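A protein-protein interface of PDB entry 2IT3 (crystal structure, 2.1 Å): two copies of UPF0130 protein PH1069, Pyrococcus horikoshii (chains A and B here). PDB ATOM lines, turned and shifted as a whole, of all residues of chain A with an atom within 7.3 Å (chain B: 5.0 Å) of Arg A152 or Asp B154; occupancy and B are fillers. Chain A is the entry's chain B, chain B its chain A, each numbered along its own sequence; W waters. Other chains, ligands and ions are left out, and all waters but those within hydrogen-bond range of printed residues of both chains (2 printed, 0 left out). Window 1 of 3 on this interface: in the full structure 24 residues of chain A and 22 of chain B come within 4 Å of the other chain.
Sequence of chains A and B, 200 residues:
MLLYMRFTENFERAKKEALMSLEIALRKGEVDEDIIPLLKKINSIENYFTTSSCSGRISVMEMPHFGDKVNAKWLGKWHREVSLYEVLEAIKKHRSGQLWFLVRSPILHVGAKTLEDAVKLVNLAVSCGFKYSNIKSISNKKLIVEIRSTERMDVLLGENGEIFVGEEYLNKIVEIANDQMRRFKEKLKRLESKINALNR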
ATOM      1  N   PHE A  66     -16.834  -5.024  -2.529  1.00  0.00           N
ATOM      2  CA  PHE A  66     -16.648  -4.339  -1.256  1.00  0.00           C
ATOM      3  C   PHE A  66     -18.000  -4.038  -0.625  1.00  0.00           C
ATOM      4  O   PHE A  66     -18.938  -3.642  -1.317  1.00  0.00           O
ATOM      5  CB  PHE A  66     -15.884  -3.030  -1.473  1.00  0.00           C
ATOM      6  CG  PHE A  66     -15.688  -2.226  -0.220  1.00  0.00           C
ATOM      7  CD1 PHE A  66     -14.753  -2.614   0.731  1.00  0.00           C
ATOM      8  CD2 PHE A  66     -16.449  -1.087   0.015  1.00  0.00           C
ATOM      9  CE1 PHE A  66     -14.577  -1.882   1.899  1.00  0.00           C
ATOM     10  CE2 PHE A  66     -16.283  -0.346   1.178  1.00  0.00           C
ATOM     11  CZ  PHE A  66     -15.341  -0.745   2.126  1.00  0.00           C
ATOM     12  N   GLY A  67     -18.102  -4.238   0.685  1.00  0.00           N
ATOM     13  CA  GLY A  67     -19.344  -3.954   1.389  1.00  0.00           C
ATOM     14  C   GLY A  67     -20.408  -5.029   1.288  1.00  0.00           C
ATOM     15  O   GLY A  67     -21.474  -4.906   1.890  1.00  0.00           O
ATOM     16  N   PHE A 101      -8.532  -6.961   3.326  1.00  0.00           N
ATOM     17  CA  PHE A 101      -7.964  -6.978   4.665  1.00  0.00           C
ATOM     18  C   PHE A 101      -8.746  -5.887   5.388  1.00  0.00           C
ATOM     19  O   PHE A 101      -8.757  -4.732   4.961  1.00  0.00           O
ATOM     20  CB  PHE A 101      -6.485  -6.629   4.634  1.00  0.00           C
ATOM     21  CG  PHE A 101      -5.871  -6.512   5.993  1.00  0.00           C
ATOM     22  CD1 PHE A 101      -5.910  -5.304   6.686  1.00  0.00           C
ATOM     23  CD2 PHE A 101      -5.255  -7.606   6.582  1.00  0.00           C
ATOM     24  CE1 PHE A 101      -5.341  -5.189   7.942  1.00  0.00           C
ATOM     25  CE2 PHE A 101      -4.682  -7.506   7.835  1.00  0.00           C
ATOM     26  CZ  PHE A 101      -4.722  -6.291   8.522  1.00  0.00           C
ATOM     27  N   LEU A 102      -9.412  -6.253   6.471  1.00  0.00           N
ATOM     28  CA  LEU A 102     -10.220  -5.295   7.206  1.00  0.00           C
ATOM     29  C   LEU A 102      -9.850  -5.156   8.665  1.00  0.00           C
ATOM     30  O   LEU A 102      -9.321  -6.081   9.283  1.00  0.00           O
ATOM     31  CB  LEU A 102     -11.699  -5.688   7.147  1.00  0.00           C
ATOM     32  CG  LEU A 102     -12.331  -6.011   5.791  1.00  0.00           C
ATOM     33  CD1 LEU A 102     -13.790  -6.382   6.013  1.00  0.00           C
ATOM     34  CD2 LEU A 102     -12.217  -4.822   4.844  1.00  0.00           C
ATOM     35  N   VAL A 103     -10.154  -3.978   9.200  1.00  0.00           N
ATOM     36  CA  VAL A 103      -9.957  -3.661  10.597  1.00  0.00           C
ATOM     37  C   VAL A 103     -11.246  -2.939  10.974  1.00  0.00           C
ATOM     38  O   VAL A 103     -11.663  -1.995  10.291  1.00  0.00           O
ATOM     39  CB  VAL A 103      -8.790  -2.706  10.830  1.00  0.00           C
ATOM     40  CG1 VAL A 103      -8.647  -2.438  12.311  1.00  0.00           C
ATOM     41  CG2 VAL A 103      -7.510  -3.294  10.269  1.00  0.00           C
ATOM     42  N   ARG A 104     -11.891  -3.409  12.034  1.00  0.00           N
ATOM     43  CA  ARG A 104     -13.130  -2.818  12.510  1.00  0.00           C
ATOM     44  C   ARG A 104     -13.013  -2.617  14.010  1.00  0.00           C
ATOM     45  O   ARG A 104     -12.407  -3.436  14.719  1.00  0.00           O
ATOM     46  CB  ARG A 104     -14.319  -3.727  12.185  1.00  0.00           C
ATOM     47  CG  ARG A 104     -14.614  -3.845  10.693  1.00  0.00           C
ATOM     48  CD  ARG A 104     -15.153  -2.526  10.143  1.00  0.00           C
ATOM     49  NE  ARG A 104     -15.562  -2.615   8.739  1.00  0.00           N
ATOM     50  CZ  ARG A 104     -14.759  -2.417   7.699  1.00  0.00           C
ATOM     51  NH1 ARG A 104     -13.488  -2.117   7.880  1.00  0.00           N
ATOM     52  NH2 ARG A 104     -15.239  -2.500   6.465  1.00  0.00           N
ATOM     53  N   SER A 105     -13.600  -1.533  14.500  1.00  0.00           N
ATOM     54  CA  SER A 105     -13.514  -1.225  15.915  1.00  0.00           C
ATOM     55  C   SER A 105     -14.497  -2.007  16.766  1.00  0.00           C
ATOM     56  O   SER A 105     -15.456  -2.568  16.259  1.00  0.00           O
ATOM     57  CB  SER A 105     -13.734   0.276  16.139  1.00  0.00           C
ATOM     58  OG  SER A 105     -15.109   0.581  16.254  1.00  0.00           O
ATOM     59  N   TYR A 132     -17.583   7.559  18.260  1.00  0.00           N
ATOM     60  CA  TYR A 132     -18.864   7.242  17.646  1.00  0.00           C
ATOM     61  C   TYR A 132     -19.910   6.685  18.612  1.00  0.00           C
ATOM     62  O   TYR A 132     -20.848   6.022  18.191  1.00  0.00           O
ATOM     63  CB  TYR A 132     -18.664   6.263  16.485  1.00  0.00           C
ATOM     64  CG  TYR A 132     -18.181   6.904  15.198  1.00  0.00           C
ATOM     65  CD1 TYR A 132     -18.307   8.281  14.992  1.00  0.00           C
ATOM     66  CD2 TYR A 132     -17.675   6.127  14.155  1.00  0.00           C
ATOM     67  CE1 TYR A 132     -17.951   8.867  13.780  1.00  0.00           C
ATOM     68  CE2 TYR A 132     -17.314   6.707  12.931  1.00  0.00           C
ATOM     69  CZ  TYR A 132     -17.458   8.078  12.754  1.00  0.00           C
ATOM     70  OH  TYR A 132     -17.133   8.662  11.551  1.00  0.00           O
ATOM     71  N   ARG A 148     -18.624   2.850  20.170  1.00  0.00           N
ATOM     72  CA  ARG A 148     -17.799   2.425  19.047  1.00  0.00           C
ATOM     73  C   ARG A 148     -16.731   3.462  18.750  1.00  0.00           C
ATOM     74  O   ARG A 148     -16.894   4.643  19.043  1.00  0.00           O
ATOM     75  CB  ARG A 148     -18.683   2.226  17.817  1.00  0.00           C
ATOM     76  CG  ARG A 148     -18.041   1.446  16.699  1.00  0.00           C
ATOM     77  CD  ARG A 148     -19.070   1.070  15.646  1.00  0.00           C
ATOM     78  NE  ARG A 148     -19.376   2.174  14.749  1.00  0.00           N
ATOM     79  CZ  ARG A 148     -18.534   2.647  13.831  1.00  0.00           C
ATOM     80  NH1 ARG A 148     -17.325   2.111  13.681  1.00  0.00           N
ATOM     81  NH2 ARG A 148     -18.905   3.658  13.054  1.00  0.00           N
ATOM     82  N   SER A 149     -15.626   3.012  18.178  1.00  0.00           N
ATOM     83  CA  SER A 149     -14.565   3.931  17.843  1.00  0.00           C
ATOM     84  C   SER A 149     -14.605   4.207  16.350  1.00  0.00           C
ATOM     85  O   SER A 149     -15.276   3.496  15.598  1.00  0.00           O
ATOM     86  CB  SER A 149     -13.211   3.362  18.233  1.00  0.00           C
ATOM     87  OG  SER A 149     -12.239   4.385  18.131  1.00  0.00           O
ATOM     88  N   THR A 150     -13.858   5.224  15.935  1.00  0.00           N
ATOM     89  CA  THR A 150     -13.800   5.663  14.546  1.00  0.00           C
ATOM     90  C   THR A 150     -12.799   4.913  13.655  1.00  0.00           C
ATOM     91  O   THR A 150     -13.029   4.746  12.460  1.00  0.00           O
ATOM     92  CB  THR A 150     -13.429   7.158  14.479  1.00  0.00           C
ATOM     93  OG1 THR A 150     -12.043   7.312  14.815  1.00  0.00           O
ATOM     94  CG2 THR A 150     -14.253   7.956  15.479  1.00  0.00           C
ATOM     95  N   GLU A 151     -11.686   4.487  14.234  1.00  0.00           N
ATOM     96  CA  GLU A 151     -10.649   3.798  13.481  1.00  0.00           C
ATOM     97  C   GLU A 151     -11.052   2.542  12.736  1.00  0.00           C
ATOM     98  O   GLU A 151     -11.748   1.690  13.268  1.00  0.00           O
ATOM     99  CB  GLU A 151      -9.468   3.457  14.393  1.00  0.00           C
ATOM    100  CG  GLU A 151      -8.330   4.455  14.331  1.00  0.00           C
ATOM    101  CD  GLU A 151      -8.749   5.852  14.751  1.00  0.00           C
ATOM    102  OE1 GLU A 151      -9.887   6.010  15.248  1.00  0.00           O
ATOM    103  OE2 GLU A 151      -7.939   6.793  14.586  1.00  0.00           O
ATOM    104  N   ARG A 152     -10.610   2.452  11.488  1.00  0.00           N
ATOM    105  CA  ARG A 152     -10.840   1.279  10.652  1.00  0.00           C
ATOM    106  C   ARG A 152      -9.867   1.269   9.480  1.00  0.00           C
ATOM    107  O   ARG A 152      -9.088   2.210   9.291  1.00  0.00           O
ATOM    108  CB  ARG A 152     -12.276   1.223  10.135  1.00  0.00           C
ATOM    109  CG  ARG A 152     -12.660   2.278   9.134  1.00  0.00           C
ATOM    110  CD  ARG A 152     -14.133   2.081   8.764  1.00  0.00           C
ATOM    111  NE  ARG A 152     -14.306   1.428   7.475  1.00  0.00           N
ATOM    112  CZ  ARG A 152     -15.357   0.682   7.146  1.00  0.00           C
ATOM    113  NH1 ARG A 152     -16.333   0.479   8.019  1.00  0.00           N
ATOM    114  NH2 ARG A 152     -15.442   0.165   5.930  1.00  0.00           N
ATOM    115  N   MET A 153      -9.892   0.184   8.715  1.00  0.00           N
ATOM    116  CA  MET A 153      -9.031   0.054   7.561  1.00  0.00           C
ATOM    117  C   MET A 153      -9.669  -0.912   6.574  1.00  0.00           C
ATOM    118  O   MET A 153     -10.300  -1.901   6.960  1.00  0.00           O
ATOM    119  CB  MET A 153      -7.642  -0.461   7.975  1.00  0.00           C
ATOM    120  CG  MET A 153      -6.595  -0.423   6.857  1.00  0.00           C
ATOM    121  SD  MET A 153      -4.838  -1.115   7.380  1.00  0.00           S
ATOM    122  CE  MET A 153      -4.988  -0.783   9.269  1.00  0.00           C
ATOM    123  N   ASP A 154      -9.503  -0.592   5.299  1.00  0.00           N
ATOM    124  CA  ASP A 154     -10.017  -1.385   4.194  1.00  0.00           C
ATOM    125  C   ASP A 154      -8.912  -1.368   3.151  1.00  0.00           C
ATOM    126  O   ASP A 154      -8.516  -0.300   2.687  1.00  0.00           O
ATOM    127  CB  ASP A 154     -11.267  -0.745   3.597  1.00  0.00           C
ATOM    128  CG  ASP A 154     -12.376  -0.567   4.611  1.00  0.00           C
ATOM    129  OD1 ASP A 154     -13.078  -1.558   4.905  1.00  0.00           O
ATOM    130  OD2 ASP A 154     -12.538   0.557   5.123  1.00  0.00           O
ATOM    131  N   VAL A 155      -8.400  -2.542   2.799  1.00  0.00           N
ATOM    132  CA  VAL A 155      -7.347  -2.641   1.800  1.00  0.00           C
ATOM    133  C   VAL A 155      -7.614  -3.825   0.864  1.00  0.00           C
ATOM    134  O   VAL A 155      -7.810  -4.956   1.316  1.00  0.00           O
ATOM    135  CB  VAL A 155      -5.961  -2.824   2.472  1.00  0.00           C
ATOM    136  CG1 VAL A 155      -4.881  -2.905   1.420  1.00  0.00           C
ATOM    137  CG2 VAL A 155      -5.682  -1.660   3.420  1.00  0.00           C
ATOM    138  N   ILE A 176       0.307  -1.249  10.881  1.00  0.00           N
ATOM    139  CA  ILE A 176      -0.712  -0.230  11.137  1.00  0.00           C
ATOM    140  C   ILE A 176      -1.943  -0.838  11.792  1.00  0.00           C
ATOM    141  O   ILE A 176      -2.476  -0.288  12.749  1.00  0.00           O
ATOM    142  CB  ILE A 176      -1.180   0.460   9.835  1.00  0.00           C
ATOM    143  CG1 ILE A 176      -0.007   1.185   9.168  1.00  0.00           C
ATOM    144  CG2 ILE A 176      -2.299   1.439  10.148  1.00  0.00           C
ATOM    145  CD1 ILE A 176       0.633   2.241  10.042  1.00  0.00           C
ATOM    146  N   GLN A 180      -3.798   0.048  15.483  1.00  0.00           N
ATOM    147  CA  GLN A 180      -5.204   0.388  15.700  1.00  0.00           C
ATOM    148  C   GLN A 180      -5.829  -0.572  16.706  1.00  0.00           C
ATOM    149  O   GLN A 180      -6.618  -0.157  17.555  1.00  0.00           O
ATOM    150  CB  GLN A 180      -5.991   0.334  14.382  1.00  0.00           C
ATOM    151  CG  GLN A 180      -5.513   1.306  13.295  1.00  0.00           C
ATOM    152  CD  GLN A 180      -6.357   1.225  12.028  1.00  0.00           C
ATOM    153  OE1 GLN A 180      -6.788   0.144  11.622  1.00  0.00           O
ATOM    154  NE2 GLN A 180      -6.591   2.369  11.396  1.00  0.00           N
ATOM    155  N   PHE A 184      -7.613   0.021  20.327  1.00  0.00           N
ATOM    156  CA  PHE A 184      -8.926  -0.489  20.733  1.00  0.00           C
ATOM    157  C   PHE A 184      -8.838  -1.115  22.130  1.00  0.00           C
ATOM    158  O   PHE A 184      -9.651  -0.804  22.999  1.00  0.00           O
ATOM    159  CB  PHE A 184      -9.474  -1.535  19.743  1.00  0.00           C
ATOM    160  CG  PHE A 184      -9.745  -0.999  18.356  1.00  0.00           C
ATOM    161  CD1 PHE A 184     -10.091   0.335  18.162  1.00  0.00           C
ATOM    162  CD2 PHE A 184      -9.685  -1.848  17.246  1.00  0.00           C
ATOM    163  CE1 PHE A 184     -10.373   0.822  16.884  1.00  0.00           C
ATOM    164  CE2 PHE A 184      -9.962  -1.379  15.970  1.00  0.00           C
ATOM    165  CZ  PHE A 184     -10.310  -0.038  15.783  1.00  0.00           C
ATOM    166  N   TRP B 100      -3.550   7.994   3.189  1.00  0.00           N
ATOM    167  CA  TRP B 100      -4.875   7.381   3.150  1.00  0.00           C
ATOM    168  C   TRP B 100      -5.789   7.914   2.061  1.00  0.00           C
ATOM    169  O   TRP B 100      -5.796   9.104   1.766  1.00  0.00           O
ATOM    170  CB  TRP B 100      -5.631   7.609   4.468  1.00  0.00           C
ATOM    171  CG  TRP B 100      -4.974   7.059   5.683  1.00  0.00           C
ATOM    172  CD1 TRP B 100      -3.964   7.631   6.399  1.00  0.00           C
ATOM    173  CD2 TRP B 100      -5.237   5.788   6.294  1.00  0.00           C
ATOM    174  NE1 TRP B 100      -3.575   6.788   7.413  1.00  0.00           N
ATOM    175  CE2 TRP B 100      -4.339   5.651   7.372  1.00  0.00           C
ATOM    176  CE3 TRP B 100      -6.143   4.749   6.032  1.00  0.00           C
ATOM    177  CZ2 TRP B 100      -4.316   4.509   8.196  1.00  0.00           C
ATOM    178  CZ3 TRP B 100      -6.122   3.614   6.850  1.00  0.00           C
ATOM    179  CH2 TRP B 100      -5.214   3.505   7.915  1.00  0.00           C
ATOM    180  N   PHE B 101      -6.579   7.019   1.484  1.00  0.00           N
ATOM    181  CA  PHE B 101      -7.577   7.402   0.504  1.00  0.00           C
ATOM    182  C   PHE B 101      -8.886   7.102   1.249  1.00  0.00           C
ATOM    183  O   PHE B 101      -9.156   5.951   1.615  1.00  0.00           O
ATOM    184  CB  PHE B 101      -7.426   6.565  -0.768  1.00  0.00           C
ATOM    185  CG  PHE B 101      -8.574   6.699  -1.725  1.00  0.00           C
ATOM    186  CD1 PHE B 101      -9.685   5.869  -1.617  1.00  0.00           C
ATOM    187  CD2 PHE B 101      -8.554   7.665  -2.726  1.00  0.00           C
ATOM    188  CE1 PHE B 101     -10.764   5.997  -2.492  1.00  0.00           C
ATOM    189  CE2 PHE B 101      -9.624   7.806  -3.605  1.00  0.00           C
ATOM    190  CZ  PHE B 101     -10.731   6.970  -3.489  1.00  0.00           C
ATOM    191  N   LEU B 102      -9.679   8.142   1.492  1.00  0.00           N
ATOM    192  CA  LEU B 102     -10.924   8.022   2.243  1.00  0.00           C
ATOM    193  C   LEU B 102     -12.212   8.263   1.463  1.00  0.00           C
ATOM    194  O   LEU B 102     -12.249   9.018   0.502  1.00  0.00           O
ATOM    195  CB  LEU B 102     -10.912   9.001   3.422  1.00  0.00           C
ATOM    196  CG  LEU B 102      -9.647   9.175   4.262  1.00  0.00           C
ATOM    197  CD1 LEU B 102      -9.878  10.309   5.245  1.00  0.00           C
ATOM    198  CD2 LEU B 102      -9.297   7.872   5.003  1.00  0.00           C
ATOM    199  N   ARG B 104     -16.099   9.090   2.639  1.00  0.00           N
ATOM    200  CA  ARG B 104     -16.944   9.397   3.783  1.00  0.00           C
ATOM    201  C   ARG B 104     -18.381   9.597   3.316  1.00  0.00           C
ATOM    202  O   ARG B 104     -18.648  10.264   2.308  1.00  0.00           O
ATOM    203  CB  ARG B 104     -16.442  10.657   4.505  1.00  0.00           C
ATOM    204  CG  ARG B 104     -15.090  10.474   5.215  1.00  0.00           C
ATOM    205  CD  ARG B 104     -15.217   9.515   6.395  1.00  0.00           C
ATOM    206  NE  ARG B 104     -13.948   9.295   7.101  1.00  0.00           N
ATOM    207  CZ  ARG B 104     -13.077   8.334   6.803  1.00  0.00           C
ATOM    208  NH1 ARG B 104     -13.323   7.499   5.803  1.00  0.00           N
ATOM    209  NH2 ARG B 104     -11.971   8.192   7.525  1.00  0.00           N
ATOM    210  N   ARG B 152     -18.434   3.512   4.018  1.00  0.00           N
ATOM    211  CA  ARG B 152     -17.174   4.157   4.352  1.00  0.00           C
ATOM    212  C   ARG B 152     -15.951   3.386   3.849  1.00  0.00           C
ATOM    213  O   ARG B 152     -15.981   2.168   3.760  1.00  0.00           O
ATOM    214  CB  ARG B 152     -17.108   4.299   5.871  1.00  0.00           C
ATOM    215  CG  ARG B 152     -15.801   4.782   6.405  1.00  0.00           C
ATOM    216  CD  ARG B 152     -15.859   4.894   7.907  1.00  0.00           C
ATOM    217  NE  ARG B 152     -14.558   5.294   8.423  1.00  0.00           N
ATOM    218  CZ  ARG B 152     -14.275   5.456   9.710  1.00  0.00           C
ATOM    219  NH1 ARG B 152     -15.211   5.248  10.636  1.00  0.00           N
ATOM    220  NH2 ARG B 152     -13.053   5.834  10.066  1.00  0.00           N
ATOM    221  N   MET B 153     -14.883   4.106   3.519  1.00  0.00           N
ATOM    222  CA  MET B 153     -13.640   3.491   3.069  1.00  0.00           C
ATOM    223  C   MET B 153     -12.432   4.199   3.664  1.00  0.00           C
ATOM    224  O   MET B 153     -12.378   5.426   3.699  1.00  0.00           O
ATOM    225  CB  MET B 153     -13.512   3.532   1.545  1.00  0.00           C
ATOM    226  CG  MET B 153     -14.287   2.467   0.804  1.00  0.00           C
ATOM    227  SD  MET B 153     -13.808   2.491  -1.061  1.00  0.00           S
ATOM    228  CE  MET B 153     -12.478   1.089  -1.031  1.00  0.00           C
ATOM    229  N   ASP B 154     -11.468   3.407   4.123  1.00  0.00           N
ATOM    230  CA  ASP B 154     -10.226   3.902   4.699  1.00  0.00           C
ATOM    231  C   ASP B 154      -9.074   3.067   4.112  1.00  0.00           C
ATOM    232  O   ASP B 154      -8.655   2.067   4.699  1.00  0.00           O
ATOM    233  CB  ASP B 154     -10.256   3.752   6.225  1.00  0.00           C
ATOM    234  CG  ASP B 154     -11.266   4.674   6.883  1.00  0.00           C
ATOM    235  OD1 ASP B 154     -12.480   4.458   6.695  1.00  0.00           O
ATOM    236  OD2 ASP B 154     -10.846   5.617   7.589  1.00  0.00           O
ATOM    237  N   VAL B 155      -8.567   3.481   2.957  1.00  0.00           N
ATOM    238  CA  VAL B 155      -7.501   2.747   2.286  1.00  0.00           C
ATOM    239  C   VAL B 155      -6.089   3.274   2.511  1.00  0.00           C
ATOM    240  O   VAL B 155      -5.781   4.414   2.167  1.00  0.00           O
ATOM    241  CB  VAL B 155      -7.751   2.698   0.763  1.00  0.00           C
ATOM    242  CG1 VAL B 155      -6.702   1.823   0.094  1.00  0.00           C
ATOM    243  CG2 VAL B 155      -9.154   2.173   0.474  1.00  0.00           C
ATOM    244  N   LEU B 156      -5.233   2.438   3.097  1.00  0.00           N
ATOM    245  CA  LEU B 156      -3.833   2.799   3.338  1.00  0.00           C
ATOM    246  C   LEU B 156      -3.113   2.621   2.008  1.00  0.00           C
ATOM    247  O   LEU B 156      -3.121   1.531   1.456  1.00  0.00           O
ATOM    248  CB  LEU B 156      -3.205   1.859   4.369  1.00  0.00           C
ATOM    249  CG  LEU B 156      -1.703   2.034   4.614  1.00  0.00           C
ATOM    250  CD1 LEU B 156      -1.450   3.272   5.497  1.00  0.00           C
ATOM    251  CD2 LEU B 156      -1.159   0.774   5.290  1.00  0.00           C
HETATM  252  O   HOH W   1     -17.971   3.742  10.799  1.00  0.00           O
HETATM  253  O   HOH W   2     -17.917   0.288   4.358  1.00  0.00           O
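OD1 of Asp B154 is in salt-bridge range of NE of Arg A152 (3.6 Å). N of Asp A154 lies within hydrogen-bond range of O of Asp B154, at 2.9 Å. The backbone carbonyl oxygen (O) of Thr A150 is in hydrogen-bond range of the guanidinium group (NH2) of Arg B152 (2.6 Å). The guanidinium group (NH2) of Arg A152 lies within hydrogen-bond range of the backbone carbonyl oxygen (O) of Arg B152, 3.0 Å away.
The side-chain hydroxyl (OG1) of Thr A150 is in hydrogen-bond range of the side-chain carboxylate (OE1) of Glu A151 (2.6 Å). The backbone NH (N) of Val A103 is in hydrogen-bond range of the backbone carbonyl oxygen (O) of Met A153, 3.1 Å away. The guanidinium group (NH2) of Arg A152 lies close to the guanidinium group (NH2) of Arg A104, 2.7 Å away. The backbone carbonyl oxygen (O) of Arg A152 sits at hydrogen-bond distance from the side-chain amide nitrogen (NE2) of Gln A180, 3.3 Å away. O of Arg A148 lies within hydrogen-bond range of N of Tyr A132. The guanidinium group of Arg A104 is in salt-bridge range of the side-chain carboxylate of Asp A154, at 2.8 Å.
Among the printed residues, merely in contact across the chains: Asp A154 with Val B155, Phe A66 with Arg B152, Tyr A132 with Arg B152, Phe A66 with Met B153, Met A153 with Asp B154, Asp A154 with Met B153 and Gln A180 with Trp B100.
Of the printed residues of chain A, Asp B154 touches Arg A152 (3.3 Å), Met A153 (3.5 Å) and Asp A154 (2.9 Å). Of the printed residues of chain B, Tyr A132 touches Arg B152 (3.4 Å). Of the printed residues of chain B, Thr A150 touches Arg B152. Of the printed residues of chain B, Asp A154 touches Met B153, Asp B154 and Val B155. Of the printed residues of chain A, Trp B100 touches Gln A180 (3.9 Å). Of the printed residues of chain A, Arg B152 touches Phe A66, Tyr A132, Thr A150 and Arg A152.
Of the 9 printed residues of chain B, 5 touch a printed residue of chain A.
Arg A152 touches its own counterpart, Arg B152. Met A153 touches Asp B154, and with the chains exchanged Asp A154 touches Met B153. Asp B154 touches its own counterpart, Asp A154. Asp A154 touches Val B155, but with the chains exchanged Val A155 does not touch Asp B154 (4.9 Å). Positions printed for both chains: 101, 102, 104, 152, 153, 154 and 155.
Water W1 bridges NH2 of Arg A148 (2.4 Å) and NH1 of Arg B152 (3.1 Å). Water W2 lies within hydrogen-bond range of the backbone carbonyl oxygen of Arg B152 (2.8 Å) and the guanidinium group of Arg A152 (2.9 Å).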
